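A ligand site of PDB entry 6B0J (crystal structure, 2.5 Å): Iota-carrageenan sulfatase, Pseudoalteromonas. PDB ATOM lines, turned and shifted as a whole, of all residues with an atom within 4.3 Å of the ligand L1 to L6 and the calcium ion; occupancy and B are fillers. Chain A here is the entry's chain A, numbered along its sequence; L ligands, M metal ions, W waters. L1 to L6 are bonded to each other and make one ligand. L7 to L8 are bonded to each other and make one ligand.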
ATOM      1  N   ASP A  11       6.855  17.538  -1.466  1.00  0.00           N
ATOM      2  CA  ASP A  11       7.252  16.285  -0.835  1.00  0.00           C
ATOM      3  C   ASP A  11       7.403  16.468   0.677  1.00  0.00           C
ATOM      4  O   ASP A  11       8.313  17.164   1.120  1.00  0.00           O
ATOM      5  CB  ASP A  11       8.587  15.846  -1.479  1.00  0.00           C
ATOM      6  CG  ASP A  11       9.032  14.455  -1.083  1.00  0.00           C
ATOM      7  OD1 ASP A  11       8.461  13.849  -0.161  1.00  0.00           O
ATOM      8  OD2 ASP A  11      10.001  13.959  -1.699  1.00  0.00           O
ATOM      9  N   ASP A  12       6.507  15.843   1.444  1.00  0.00           N
ATOM     10  CA  ASP A  12       6.421  15.990   2.912  1.00  0.00           C
ATOM     11  C   ASP A  12       5.969  17.397   3.361  1.00  0.00           C
ATOM     12  O   ASP A  12       6.275  17.829   4.494  1.00  0.00           O
ATOM     13  CB  ASP A  12       7.739  15.605   3.636  1.00  0.00           C
ATOM     14  CG  ASP A  12       8.061  14.115   3.571  1.00  0.00           C
ATOM     15  OD1 ASP A  12       7.267  13.316   3.024  1.00  0.00           O
ATOM     16  OD2 ASP A  12       9.118  13.719   4.090  1.00  0.00           O
ATOM     17  N   PRO A  49      -0.055   7.219   3.014  1.00  0.00           N
ATOM     18  CA  PRO A  49       0.601   8.255   3.818  1.00  0.00           C
ATOM     19  C   PRO A  49       2.120   8.405   3.652  1.00  0.00           C
ATOM     20  O   PRO A  49       2.770   9.012   4.497  1.00  0.00           O
ATOM     21  CB  PRO A  49       0.233   7.861   5.249  1.00  0.00           C
ATOM     22  CG  PRO A  49       0.103   6.370   5.200  1.00  0.00           C
ATOM     23  CD  PRO A  49      -0.484   6.077   3.842  1.00  0.00           C
ATOM     24  N   PHE A  50       2.683   7.871   2.564  1.00  0.00           N
ATOM     25  CA  PHE A  50       4.061   8.207   2.172  1.00  0.00           C
ATOM     26  C   PHE A  50       4.312   8.048   0.667  1.00  0.00           C
ATOM     27  O   PHE A  50       3.441   7.589  -0.066  1.00  0.00           O
ATOM     28  CB  PHE A  50       5.109   7.509   3.051  1.00  0.00           C
ATOM     29  CG  PHE A  50       5.084   6.006   3.024  1.00  0.00           C
ATOM     30  CD1 PHE A  50       5.610   5.319   1.956  1.00  0.00           C
ATOM     31  CD2 PHE A  50       4.602   5.283   4.110  1.00  0.00           C
ATOM     32  CE1 PHE A  50       5.629   3.934   1.930  1.00  0.00           C
ATOM     33  CE2 PHE A  50       4.608   3.887   4.110  1.00  0.00           C
ATOM     34  CZ  PHE A  50       5.113   3.204   3.007  1.00  0.00           C
ATOM     35  N   SER A  51       5.519   8.436   0.237  1.00  0.00           N
ATOM     36  CA  SER A  51       5.819   8.862  -1.139  1.00  0.00           C
ATOM     37  C   SER A  51       5.534   7.932  -2.301  1.00  0.00           C
ATOM     38  O   SER A  51       4.735   8.267  -3.181  1.00  0.00           O
ATOM     39  CB  SER A  51       7.296   9.235  -1.217  1.00  0.00           C
ATOM     40  OG  SER A  51       7.673   9.606  -2.515  1.00  0.00           O
ATOM     41  N   ASN A  72       7.690   1.827  -0.381  1.00  0.00           N
ATOM     42  CA  ASN A  72       8.705   2.560  -1.124  1.00  0.00           C
ATOM     43  C   ASN A  72       9.686   1.569  -1.746  1.00  0.00           C
ATOM     44  O   ASN A  72       9.945   0.498  -1.172  1.00  0.00           O
ATOM     45  CB  ASN A  72       9.477   3.525  -0.226  1.00  0.00           C
ATOM     46  CG  ASN A  72       8.701   4.781   0.122  1.00  0.00           C
ATOM     47  OD1 ASN A  72       7.705   5.119  -0.516  1.00  0.00           O
ATOM     48  ND2 ASN A  72       9.164   5.507   1.144  1.00  0.00           N
ATOM     49  N   LYS A 105      11.530  14.655  -8.729  1.00  0.00           N
ATOM     50  CA  LYS A 105      11.460  13.344  -8.082  1.00  0.00           C
ATOM     51  C   LYS A 105      10.574  12.380  -8.852  1.00  0.00           C
ATOM     52  O   LYS A 105       9.465  12.736  -9.233  1.00  0.00           O
ATOM     53  CB  LYS A 105      10.922  13.495  -6.657  1.00  0.00           C
ATOM     54  CG  LYS A 105      10.842  12.207  -5.872  1.00  0.00           C
ATOM     55  CD  LYS A 105      10.640  12.469  -4.385  1.00  0.00           C
ATOM     56  CE  LYS A 105      10.148  11.210  -3.695  1.00  0.00           C
ATOM     57  NZ  LYS A 105      10.044  11.340  -2.224  1.00  0.00           N
ATOM     58  N   HIS A 107      10.759   8.285  -8.123  1.00  0.00           N
ATOM     59  CA  HIS A 107      10.442   7.308  -7.051  1.00  0.00           C
ATOM     60  C   HIS A 107       9.452   6.231  -7.503  1.00  0.00           C
ATOM     61  O   HIS A 107       8.664   5.720  -6.703  1.00  0.00           O
ATOM     62  CB  HIS A 107       9.939   8.056  -5.792  1.00  0.00           C
ATOM     63  CG  HIS A 107      10.292   7.379  -4.497  1.00  0.00           C
ATOM     64  ND1 HIS A 107       9.610   7.646  -3.321  1.00  0.00           N
ATOM     65  CD2 HIS A 107      11.248   6.469  -4.183  1.00  0.00           C
ATOM     66  CE1 HIS A 107      10.135   6.928  -2.342  1.00  0.00           C
ATOM     67  NE2 HIS A 107      11.132   6.214  -2.834  1.00  0.00           N
ATOM     68  N   GLY A 130      14.275   8.541  -4.250  1.00  0.00           N
ATOM     69  CA  GLY A 130      13.376   9.059  -3.221  1.00  0.00           C
ATOM     70  C   GLY A 130      13.610  10.492  -2.781  1.00  0.00           C
ATOM     71  O   GLY A 130      12.806  11.075  -2.060  1.00  0.00           O
ATOM     72  N   GLY A 131      14.736  11.063  -3.212  1.00  0.00           N
ATOM     73  CA  GLY A 131      15.051  12.448  -2.912  1.00  0.00           C
ATOM     74  C   GLY A 131      16.431  12.793  -3.418  1.00  0.00           C
ATOM     75  O   GLY A 131      17.039  12.038  -4.199  1.00  0.00           O
ATOM     76  N   PHE A 155      24.853   6.339  -2.683  1.00  0.00           N
ATOM     77  CA  PHE A 155      23.643   6.934  -2.149  1.00  0.00           C
ATOM     78  C   PHE A 155      22.995   7.833  -3.201  1.00  0.00           C
ATOM     79  O   PHE A 155      23.636   8.760  -3.705  1.00  0.00           O
ATOM     80  CB  PHE A 155      24.009   7.730  -0.886  1.00  0.00           C
ATOM     81  CG  PHE A 155      22.847   8.378  -0.187  1.00  0.00           C
ATOM     82  CD1 PHE A 155      21.605   7.724  -0.066  1.00  0.00           C
ATOM     83  CD2 PHE A 155      23.006   9.625   0.397  1.00  0.00           C
ATOM     84  CE1 PHE A 155      20.558   8.324   0.602  1.00  0.00           C
ATOM     85  CE2 PHE A 155      21.956  10.235   1.068  1.00  0.00           C
ATOM     86  CZ  PHE A 155      20.727   9.591   1.161  1.00  0.00           C
ATOM     87  N   TYR A 157      20.970  10.182  -3.365  1.00  0.00           N
ATOM     88  CA  TYR A 157      20.837  11.621  -3.094  1.00  0.00           C
ATOM     89  C   TYR A 157      22.004  12.504  -3.576  1.00  0.00           C
ATOM     90  O   TYR A 157      21.833  13.726  -3.683  1.00  0.00           O
ATOM     91  CB  TYR A 157      20.642  11.879  -1.587  1.00  0.00           C
ATOM     92  CG  TYR A 157      19.226  11.681  -1.070  1.00  0.00           C
ATOM     93  CD1 TYR A 157      18.567  12.717  -0.389  1.00  0.00           C
ATOM     94  CD2 TYR A 157      18.551  10.471  -1.246  1.00  0.00           C
ATOM     95  CE1 TYR A 157      17.283  12.550   0.094  1.00  0.00           C
ATOM     96  CE2 TYR A 157      17.262  10.295  -0.773  1.00  0.00           C
ATOM     97  CZ  TYR A 157      16.633  11.331  -0.107  1.00  0.00           C
ATOM     98  OH  TYR A 157      15.353  11.178   0.373  1.00  0.00           O
ATOM     99  N   HIS A 206      11.267  17.932   1.746  1.00  0.00           N
ATOM    100  CA  HIS A 206      11.748  16.645   2.263  1.00  0.00           C
ATOM    101  C   HIS A 206      13.205  16.771   2.684  1.00  0.00           C
ATOM    102  O   HIS A 206      13.945  17.592   2.149  1.00  0.00           O
ATOM    103  CB  HIS A 206      11.633  15.583   1.155  1.00  0.00           C
ATOM    104  CG  HIS A 206      11.904  14.178   1.598  1.00  0.00           C
ATOM    105  ND1 HIS A 206      13.163  13.705   1.840  1.00  0.00           N
ATOM    106  CD2 HIS A 206      11.065  13.126   1.747  1.00  0.00           C
ATOM    107  CE1 HIS A 206      13.101  12.428   2.167  1.00  0.00           C
ATOM    108  NE2 HIS A 206      11.834  12.047   2.118  1.00  0.00           N
ATOM    109  N   THR A 207      13.608  15.931   3.643  1.00  0.00           N
ATOM    110  CA  THR A 207      14.998  15.849   4.100  1.00  0.00           C
ATOM    111  C   THR A 207      15.974  15.602   2.926  1.00  0.00           C
ATOM    112  O   THR A 207      15.572  15.016   1.917  1.00  0.00           O
ATOM    113  CB  THR A 207      15.171  14.719   5.129  1.00  0.00           C
ATOM    114  OG1 THR A 207      14.700  13.496   4.562  1.00  0.00           O
ATOM    115  CG2 THR A 207      14.389  14.998   6.406  1.00  0.00           C
ATOM    116  N   ASP A 264       2.499  15.105  -1.499  1.00  0.00           N
ATOM    117  CA  ASP A 264       2.408  13.655  -1.699  1.00  0.00           C
ATOM    118  C   ASP A 264       1.924  12.948  -0.441  1.00  0.00           C
ATOM    119  O   ASP A 264       1.312  11.888  -0.522  1.00  0.00           O
ATOM    120  CB  ASP A 264       3.728  13.051  -2.217  1.00  0.00           C
ATOM    121  CG  ASP A 264       4.847  13.058  -1.201  1.00  0.00           C
ATOM    122  OD1 ASP A 264       4.833  13.831  -0.208  1.00  0.00           O
ATOM    123  OD2 ASP A 264       5.794  12.278  -1.415  1.00  0.00           O
ATOM    124  N   ASN A 265       2.231  13.521   0.722  1.00  0.00           N
ATOM    125  CA  ASN A 265       1.775  12.998   1.997  1.00  0.00           C
ATOM    126  C   ASN A 265       1.848  14.093   3.064  1.00  0.00           C
ATOM    127  O   ASN A 265       2.254  15.236   2.800  1.00  0.00           O
ATOM    128  CB  ASN A 265       2.589  11.767   2.379  1.00  0.00           C
ATOM    129  CG  ASN A 265       4.081  12.011   2.355  1.00  0.00           C
ATOM    130  OD1 ASN A 265       4.795  11.424   1.526  1.00  0.00           O
ATOM    131  ND2 ASN A 265       4.577  12.855   3.245  1.00  0.00           N
ATOM    132  N   LYS A 282       3.347  12.368   8.755  1.00  0.00           N
ATOM    133  CA  LYS A 282       3.819  11.458   7.711  1.00  0.00           C
ATOM    134  C   LYS A 282       3.784   9.970   8.135  1.00  0.00           C
ATOM    135  O   LYS A 282       4.286   9.606   9.200  1.00  0.00           O
ATOM    136  CB  LYS A 282       5.257  11.816   7.331  1.00  0.00           C
ATOM    137  CG  LYS A 282       5.795  11.103   6.095  1.00  0.00           C
ATOM    138  CD  LYS A 282       7.270  11.409   5.904  1.00  0.00           C
ATOM    139  CE  LYS A 282       7.856  10.607   4.760  1.00  0.00           C
ATOM    140  NZ  LYS A 282       9.298  10.897   4.560  1.00  0.00           N
ATOM    141  N   GLY A 283       3.188   9.146   7.274  1.00  0.00           N
ATOM    142  CA  GLY A 283       3.120   7.699   7.476  1.00  0.00           C
ATOM    143  C   GLY A 283       1.934   7.182   8.282  1.00  0.00           C
ATOM    144  O   GLY A 283       1.701   5.953   8.312  1.00  0.00           O
ATOM    145  N   ARG A 360      -1.660   1.269   5.507  1.00  0.00           N
ATOM    146  CA  ARG A 360      -0.210   1.372   5.608  1.00  0.00           C
ATOM    147  C   ARG A 360       0.291   0.234   6.463  1.00  0.00           C
ATOM    148  O   ARG A 360      -0.136   0.085   7.602  1.00  0.00           O
ATOM    149  CB  ARG A 360       0.208   2.717   6.231  1.00  0.00           C
ATOM    150  CG  ARG A 360       1.726   2.892   6.407  1.00  0.00           C
ATOM    151  CD  ARG A 360       2.205   2.578   7.822  1.00  0.00           C
ATOM    152  NE  ARG A 360       3.652   2.372   7.879  1.00  0.00           N
ATOM    153  CZ  ARG A 360       4.582   3.332   7.878  1.00  0.00           C
ATOM    154  NH1 ARG A 360       5.856   3.002   7.923  1.00  0.00           N
ATOM    155  NH2 ARG A 360       4.260   4.629   7.826  1.00  0.00           N
ATOM    156  N   ARG A 362       2.927  -2.237   8.637  1.00  0.00           N
ATOM    157  CA  ARG A 362       3.951  -2.139   9.666  1.00  0.00           C
ATOM    158  C   ARG A 362       4.444  -3.568   9.970  1.00  0.00           C
ATOM    159  O   ARG A 362       4.146  -4.492   9.205  1.00  0.00           O
ATOM    160  CB  ARG A 362       3.380  -1.406  10.879  1.00  0.00           C
ATOM    161  CG  ARG A 362       3.059   0.063  10.587  1.00  0.00           C
ATOM    162  CD  ARG A 362       2.768   0.865  11.845  1.00  0.00           C
ATOM    163  NE  ARG A 362       2.354   2.238  11.545  1.00  0.00           N
ATOM    164  CZ  ARG A 362       3.157   3.274  11.262  1.00  0.00           C
ATOM    165  NH1 ARG A 362       4.480   3.116  11.189  1.00  0.00           N
ATOM    166  NH2 ARG A 362       2.629   4.482  11.033  1.00  0.00           N
ATOM    167  N   LYS A 363       5.234  -3.741  11.031  1.00  0.00           N
ATOM    168  CA  LYS A 363       5.834  -5.042  11.357  1.00  0.00           C
ATOM    169  C   LYS A 363       4.791  -5.951  12.011  1.00  0.00           C
ATOM    170  O   LYS A 363       4.500  -5.824  13.203  1.00  0.00           O
ATOM    171  CB  LYS A 363       7.067  -4.891  12.261  1.00  0.00           C
ATOM    172  CG  LYS A 363       7.866  -6.188  12.443  1.00  0.00           C
ATOM    173  CD  LYS A 363       8.930  -6.085  13.530  1.00  0.00           C
ATOM    174  CE  LYS A 363      10.058  -5.139  13.131  1.00  0.00           C
ATOM    175  NZ  LYS A 363      11.098  -4.960  14.188  1.00  0.00           N
ATOM    176  N   HIS A 429      11.035  -1.618   0.891  1.00  0.00           N
ATOM    177  CA  HIS A 429      12.080  -0.559   0.906  1.00  0.00           C
ATOM    178  C   HIS A 429      13.409  -1.039   1.517  1.00  0.00           C
ATOM    179  O   HIS A 429      14.442  -0.438   1.280  1.00  0.00           O
ATOM    180  CB  HIS A 429      11.554   0.739   1.570  1.00  0.00           C
ATOM    181  CG  HIS A 429      11.801   0.830   3.041  1.00  0.00           C
ATOM    182  ND1 HIS A 429      11.118   0.058   3.959  1.00  0.00           N
ATOM    183  CD2 HIS A 429      12.626   1.630   3.770  1.00  0.00           C
ATOM    184  CE1 HIS A 429      11.534   0.356   5.178  1.00  0.00           C
ATOM    185  NE2 HIS A 429      12.437   1.321   5.092  1.00  0.00           N
ATOM    186  N   GLU A 433      12.552  -5.838   5.930  1.00  0.00           N
ATOM    187  CA  GLU A 433      11.118  -5.594   5.860  1.00  0.00           C
ATOM    188  C   GLU A 433      10.373  -6.718   5.102  1.00  0.00           C
ATOM    189  O   GLU A 433       9.324  -7.186   5.542  1.00  0.00           O
ATOM    190  CB  GLU A 433      10.824  -4.249   5.184  1.00  0.00           C
ATOM    191  CG  GLU A 433       9.403  -3.759   5.361  1.00  0.00           C
ATOM    192  CD  GLU A 433       9.225  -2.345   4.852  1.00  0.00           C
ATOM    193  OE1 GLU A 433       9.712  -2.060   3.739  1.00  0.00           O
ATOM    194  OE2 GLU A 433       8.589  -1.525   5.564  1.00  0.00           O
HETATM  195  C1  LIG L   1      22.098   6.126   4.611  1.00  0.00           C
HETATM  196  C2  LIG L   1      20.957   6.834   5.347  1.00  0.00           C
HETATM  197  C3  LIG L   1      20.696   8.235   4.808  1.00  0.00           C
HETATM  198  C4  LIG L   1      22.008   9.029   4.634  1.00  0.00           C
HETATM  199  C5  LIG L   1      23.038   8.181   3.880  1.00  0.00           C
HETATM  200  C6  LIG L   1      24.364   8.887   3.689  1.00  0.00           C
HETATM  201  O1  LIG L   1      22.401   4.922   5.324  1.00  0.00           O
HETATM  202  O2  LIG L   1      19.736   6.099   5.190  1.00  0.00           O
HETATM  203  O3  LIG L   1      19.777   8.877   5.717  1.00  0.00           O
HETATM  204  O4  LIG L   1      22.504   9.440   5.902  1.00  0.00           O
HETATM  205  O5  LIG L   1      23.262   6.945   4.558  1.00  0.00           O
HETATM  206  O6  LIG L   1      25.167   8.090   2.810  1.00  0.00           O
HETATM  207  S1  LIG L   1      22.428  10.919   6.357  1.00  0.00           S
HETATM  208  O7  LIG L   1      21.150  11.503   6.078  1.00  0.00           O
HETATM  209  O8  LIG L   1      22.674  10.993   7.772  1.00  0.00           O
HETATM  210  O9  LIG L   1      23.520  11.764   5.509  1.00  0.00           O
HETATM  211  C1  LG2 L   2      17.954  10.420   6.118  1.00  0.00           C
HETATM  212  C2  LG2 L   2      15.894   9.788   4.919  1.00  0.00           C
HETATM  213  C3  LG2 L   2      16.777   9.689   3.700  1.00  0.00           C
HETATM  214  C4  LG2 L   2      17.000  11.147   3.328  1.00  0.00           C
HETATM  215  O1  LG2 L   2      14.541  10.172   4.642  1.00  0.00           O
HETATM  216  O2  LG2 L   2      17.974   9.030   4.101  1.00  0.00           O
HETATM  217  O3  LG2 L   2      16.877  11.860   4.557  1.00  0.00           O
HETATM  218  C5  LG2 L   2      16.624  10.920   5.592  1.00  0.00           C
HETATM  219  O4  LG2 L   2      17.677   9.520   7.179  1.00  0.00           O
HETATM  220  C6  LG2 L   2      18.805   9.719   5.049  1.00  0.00           C
HETATM  221  C1  LG3 L   3      13.798   9.116   4.026  1.00  0.00           C
HETATM  222  C2  LG3 L   3      12.448   8.987   4.705  1.00  0.00           C
HETATM  223  C3  LG3 L   3      11.640   7.905   4.011  1.00  0.00           C
HETATM  224  C4  LG3 L   3      11.477   8.242   2.532  1.00  0.00           C
HETATM  225  C5  LG3 L   3      12.900   8.359   1.965  1.00  0.00           C
HETATM  226  C6  LG3 L   3      12.925   8.671   0.481  1.00  0.00           C
HETATM  227  O1  LG3 L   3      12.634   8.682   6.088  1.00  0.00           O
HETATM  228  O2  LG3 L   3      10.358   7.740   4.648  1.00  0.00           O
HETATM  229  O3  LG3 L   3      10.672   9.417   2.326  1.00  0.00           O
HETATM  230  O4  LG3 L   3      13.614   9.377   2.653  1.00  0.00           O
HETATM  231  O5  LG3 L   3      14.287   8.598   0.086  1.00  0.00           O
HETATM  232  S1  LG3 L   3       9.451   9.338   1.397  1.00  0.00           S
HETATM  233  O6  LG3 L   3       8.572  10.706   1.354  1.00  0.00           O
HETATM  234  O7  LG3 L   3       8.563   8.327   1.865  1.00  0.00           O
HETATM  235  O8  LG3 L   3       9.934   9.008   0.110  1.00  0.00           O
HETATM  236  C1  LG4 L   4       9.973   6.356   4.717  1.00  0.00           C
HETATM  237  C2  LG4 L   4       8.550   6.246   5.256  1.00  0.00           C
HETATM  238  C3  LG4 L   4       8.240   4.787   5.631  1.00  0.00           C
HETATM  239  C4  LG4 L   4       9.254   4.268   6.645  1.00  0.00           C
HETATM  240  C5  LG4 L   4      10.435   4.196   5.723  1.00  0.00           C
HETATM  241  C6  LG4 L   4       9.809   3.538   4.497  1.00  0.00           C
HETATM  242  O1  LG4 L   4       8.452   7.137   6.363  1.00  0.00           O
HETATM  243  O2  LG4 L   4       8.433   3.987   4.472  1.00  0.00           O
HETATM  244  O3  LG4 L   4       8.944   2.972   7.166  1.00  0.00           O
HETATM  245  O4  LG4 L   4      10.871   5.538   5.503  1.00  0.00           O
HETATM  246  O5  LG4 L   4       7.234   8.673   7.830  1.00  0.00           O
HETATM  247  O6  LG4 L   4       6.927   6.375   8.117  1.00  0.00           O
HETATM  248  O7  LG4 L   4       5.902   7.414   6.114  1.00  0.00           O
HETATM  249  S1  LG4 L   4       7.145   7.417   7.147  1.00  0.00           S
HETATM  250  C1  LG5 L   5       9.735   2.635   8.323  1.00  0.00           C
HETATM  251  C2  LG5 L   5       8.845   2.641   9.562  1.00  0.00           C
HETATM  252  C3  LG5 L   5       9.555   2.064  10.783  1.00  0.00           C
HETATM  253  C4  LG5 L   5      10.201   0.714  10.422  1.00  0.00           C
HETATM  254  C5  LG5 L   5      11.119   0.856   9.214  1.00  0.00           C
HETATM  255  C6  LG5 L   5      11.802  -0.463   8.816  1.00  0.00           C
HETATM  256  O1  LG5 L   5       8.395   3.970   9.866  1.00  0.00           O
HETATM  257  O2  LG5 L   5       8.606   2.001  11.867  1.00  0.00           O
HETATM  258  O3  LG5 L   5       9.208  -0.281  10.101  1.00  0.00           O
HETATM  259  O4  LG5 L   5      10.339   1.350   8.119  1.00  0.00           O
HETATM  260  O5  LG5 L   5      12.949  -0.200   8.004  1.00  0.00           O
HETATM  261  S1  LG5 L   5       9.059  -1.638  10.841  1.00  0.00           S
HETATM  262  O6  LG5 L   5       8.577  -2.754   9.747  1.00  0.00           O
HETATM  263  O7  LG5 L   5       8.051  -1.510  11.875  1.00  0.00           O
HETATM  264  O8  LG5 L   5      10.304  -2.061  11.397  1.00  0.00           O
HETATM  265  C1  LG6 L   6       8.354   1.609  14.303  1.00  0.00           C
HETATM  266  C2  LG6 L   6       9.018   3.481  15.808  1.00  0.00           C
HETATM  267  C3  LG6 L   6      10.162   3.711  14.842  1.00  0.00           C
HETATM  268  C4  LG6 L   6      11.161   2.640  15.280  1.00  0.00           C
HETATM  269  O1  LG6 L   6       9.312   3.843  17.150  1.00  0.00           O
HETATM  270  O2  LG6 L   6       9.658   3.520  13.500  1.00  0.00           O
HETATM  271  O3  LG6 L   6      10.327   1.553  15.763  1.00  0.00           O
HETATM  272  C5  LG6 L   6       8.948   1.966  15.670  1.00  0.00           C
HETATM  273  O4  LG6 L   6       7.023   2.121  14.205  1.00  0.00           O
HETATM  274  C6  LG6 L   6       9.243   2.160  13.173  1.00  0.00           C
HETATM  275  C1  LG7 L   7      22.662  15.299  10.053  1.00  0.00           C
HETATM  276  C2  LG7 L   7      21.736  14.348  10.816  1.00  0.00           C
HETATM  277  C3  LG7 L   7      21.296  13.188   9.922  1.00  0.00           C
HETATM  278  C4  LG7 L   7      20.690  13.710   8.609  1.00  0.00           C
HETATM  279  C5  LG7 L   7      21.668  14.704   7.936  1.00  0.00           C
HETATM  280  C6  LG7 L   7      21.094  15.329   6.664  1.00  0.00           C
HETATM  281  O1  LG7 L   7      22.999  16.447  10.854  1.00  0.00           O
HETATM  282  O2  LG7 L   7      22.411  13.832  11.975  1.00  0.00           O
HETATM  283  O3  LG7 L   7      20.366  12.346  10.633  1.00  0.00           O
HETATM  284  O4  LG7 L   7      19.379  14.279   8.832  1.00  0.00           O
HETATM  285  O5  LG7 L   7      22.033  15.754   8.848  1.00  0.00           O
HETATM  286  O6  LG7 L   7      22.021  16.204   6.027  1.00  0.00           O
HETATM  287  S1  LG7 L   7      18.120  14.024   7.968  1.00  0.00           S
HETATM  288  O7  LG7 L   7      17.550  12.740   8.281  1.00  0.00           O
HETATM  289  O8  LG7 L   7      17.160  15.058   8.257  1.00  0.00           O
HETATM  290  O9  LG7 L   7      18.421  14.087   6.358  1.00  0.00           O
HETATM  291  C1  LG8 L   8      20.336  10.978  10.145  1.00  0.00           C
HETATM  292  C2  LG8 L   8      19.030  10.280  10.600  1.00  0.00           C
HETATM  293  C3  LG8 L   8      19.189   8.755  10.671  1.00  0.00           C
HETATM  294  C4  LG8 L   8      20.389   8.449  11.544  1.00  0.00           C
HETATM  295  C5  LG8 L   8      21.447   8.803  10.510  1.00  0.00           C
HETATM  296  C6  LG8 L   8      20.901   8.244   9.191  1.00  0.00           C
HETATM  297  O1  LG8 L   8      18.583  10.795  11.869  1.00  0.00           O
HETATM  298  O2  LG8 L   8      19.480   8.256   9.360  1.00  0.00           O
HETATM  299  O3  LG8 L   8      20.429   7.090  12.036  1.00  0.00           O
HETATM  300  O4  LG8 L   8      21.556  10.239  10.465  1.00  0.00           O
HETATM  301  O5  LG8 L   8      16.205  10.847  11.313  1.00  0.00           O
HETATM  302  O6  LG8 L   8      16.878  11.499  13.472  1.00  0.00           O
HETATM  303  O7  LG8 L   8      16.934   9.068  12.937  1.00  0.00           O
HETATM  304  S1  LG8 L   8      17.139  10.590  12.384  1.00  0.00           S
HETATM  305 CA    CA M   1       7.000  12.372   0.864  1.00  0.00          CA
HETATM  306  O   HOH W   1       8.175   1.717   2.608  1.00  0.00           O
HETATM  307  O   HOH W   2       7.038  -2.208   7.515  1.00  0.00           O
HETATM  308  O   HOH W   3       9.891   9.598   7.081  1.00  0.00           O
HETATM  309  O   HOH W   4      12.112   4.902   1.754  1.00  0.00           O
HETATM  310  O   HOH W   5       6.320   0.238   8.406  1.00  0.00           O
HETATM  311  O   HOH W   6       8.933   8.710   9.909  1.00  0.00           O
HETATM  312  O   HOH W   7       8.787  -5.231   8.814  1.00  0.00           O
HETATM  313  O   HOH W   8       6.215   5.694  10.999  1.00  0.00           O
HETATM  314  O   HOH W   9      12.761  10.714   7.683  1.00  0.00           O
HETATM  315  O   HOH W  10       7.777   0.770   4.955  1.00  0.00           O
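Residues that only touch the calcium ion: Ser 51.
Within 4 Å of the calcium ion: Asp 11, Asp 12, Ser 51, Asp 264 and Asn 265.
Water W2 bridges the side-chain carboxylate of Glu 433 (2.6 Å) and an oxygen (O6) of LG5 L5 (2.8 Å).
Water W3 lies within hydrogen-bond range of NZ of Lys 282 (2.9 Å) and O5 of LG4 L4 (2.9 Å).
Water W1 bridges an oxygen (O2) of LG4 L4 (2.9 Å) and the backbone NH (N) of Asn 72 (3.0 Å).
Water W8 bridges an oxygen (O1) of LG5 L5 (3.0 Å) and the guanidinium group (NH1) of Arg 362 (3.1 Å).
Water W10 bridges the side-chain carboxylate of Glu 433 (2.5 Å) and an oxygen (O2) of LG4 L4 (3.3 Å).
Water W5 bridges the guanidinium group (NH1) of Arg 360 and an oxygen (O3) of LG5 L5.
Residues that only touch the ligand L1 to L6: Phe 50 (3.2 Å), His 107 (3.2 Å), Gly 130 (3.5 Å), Lys 363 (3.5 Å), Phe 155 (3.6 Å) and Pro 49 (3.9 Å).
Hydrophobic or aromatic side chains within 4 Å of the ligand L1 to L6: Phe 50, His 107, Phe 155, Tyr 157, His 206 and His 429.
19 residues have an atom within 4 Å of the ligand L1 to L6: Asp 11, Asp 12, Pro 49, Phe 50, Ser 51, Asn 72, Lys 105, His 107, Gly 130, Phe 155, Tyr 157, His 206, Thr 207, Asn 265, Lys 282, Gly 283, Arg 360, Lys 363 and His 429.
The nearest printed residue that does not touch the ligand L1 to L6 is Arg 362 (4.1 Å).
The calcium ion is bound by the side-chain carboxylate (OD1) of Asp 11, an oxygen (O6) of LG3 L3, the side-chain carboxylate (OD1) of Asp 12, the side-chain amide oxygen (OD1) of Asn 265, the side-chain carboxylate (OD2) of Asp 264 and the side-chain carboxylate (OD1) of Asp 264.
O3 of LG2 L2 lies within hydrogen-bond range of OG1 of Thr 207 (2.7 Å).
OH of Tyr 157 is in hydrogen-bond range of O5 of LG3 L3, 2.8 Å away.
An oxygen (O3) of LG3 L3 sits at hydrogen-bond distance from a ring nitrogen (NE2) of His 206 (2.9 Å).
The backbone NH (N) of Ser 51 sits close to an oxygen (O7) of LG3 L3 (3.5 Å).
An oxygen (O7) of LG3 L3 is in hydrogen-bond range of the side-chain amide nitrogen (ND2) of Asn 72, at 3.0 Å.
The side-chain amino group (NZ) of Lys 282 is in salt-bridge range of an oxygen (O7) of LG3 L3.
An oxygen (O7) of LG4 L4 lies close to the backbone NH (N) of Gly 283 (3.4 Å).
The guanidinium group of Arg 360 is in salt-bridge range of an oxygen (O6) of LG4 L4, 3.2 Å away.
NE2 of His 429 sits close to O5 of LG5 L5 (3.3 Å).
NZ of Lys 105 lies within salt-bridge range of O8 of LG3 L3 (3.3 Å).
The side-chain carboxylate of Asp 11 lies within salt-bridge range of the side-chain amino group of Lys 105 (2.7 Å).
N of Ser 51 sits close to OD1 of Asn 265 (3.3 Å).
The side-chain hydroxyl (OG) of Ser 51 lies close to the side-chain carboxylate (OD2) of Asp 264 (3.4 Å).
The side-chain hydroxyl (OG1) of Thr 207 lies close to a ring nitrogen (ND1) of His 206 (3.1 Å).
The side-chain hydroxyl (OG) of Ser 51 sits at hydrogen-bond distance from a ring nitrogen (ND1) of His 107, 2.9 Å away.
The backbone carbonyl oxygen (O) of Asn 72 is in hydrogen-bond range of the backbone NH (N) of His 429, 3.1 Å away.
The backbone carbonyl oxygen of Gly 283 is in hydrogen-bond range of the guanidinium group of Arg 362, 3.2 Å away.
The side-chain amino group of Lys 105 sits at hydrogen-bond distance from the backbone carbonyl oxygen of Gly 130 (2.8 Å).
An oxygen (O4) of LG2 L2 lies within hydrogen-bond range of an oxygen (O2) of LG8 L8 (3.1 Å).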
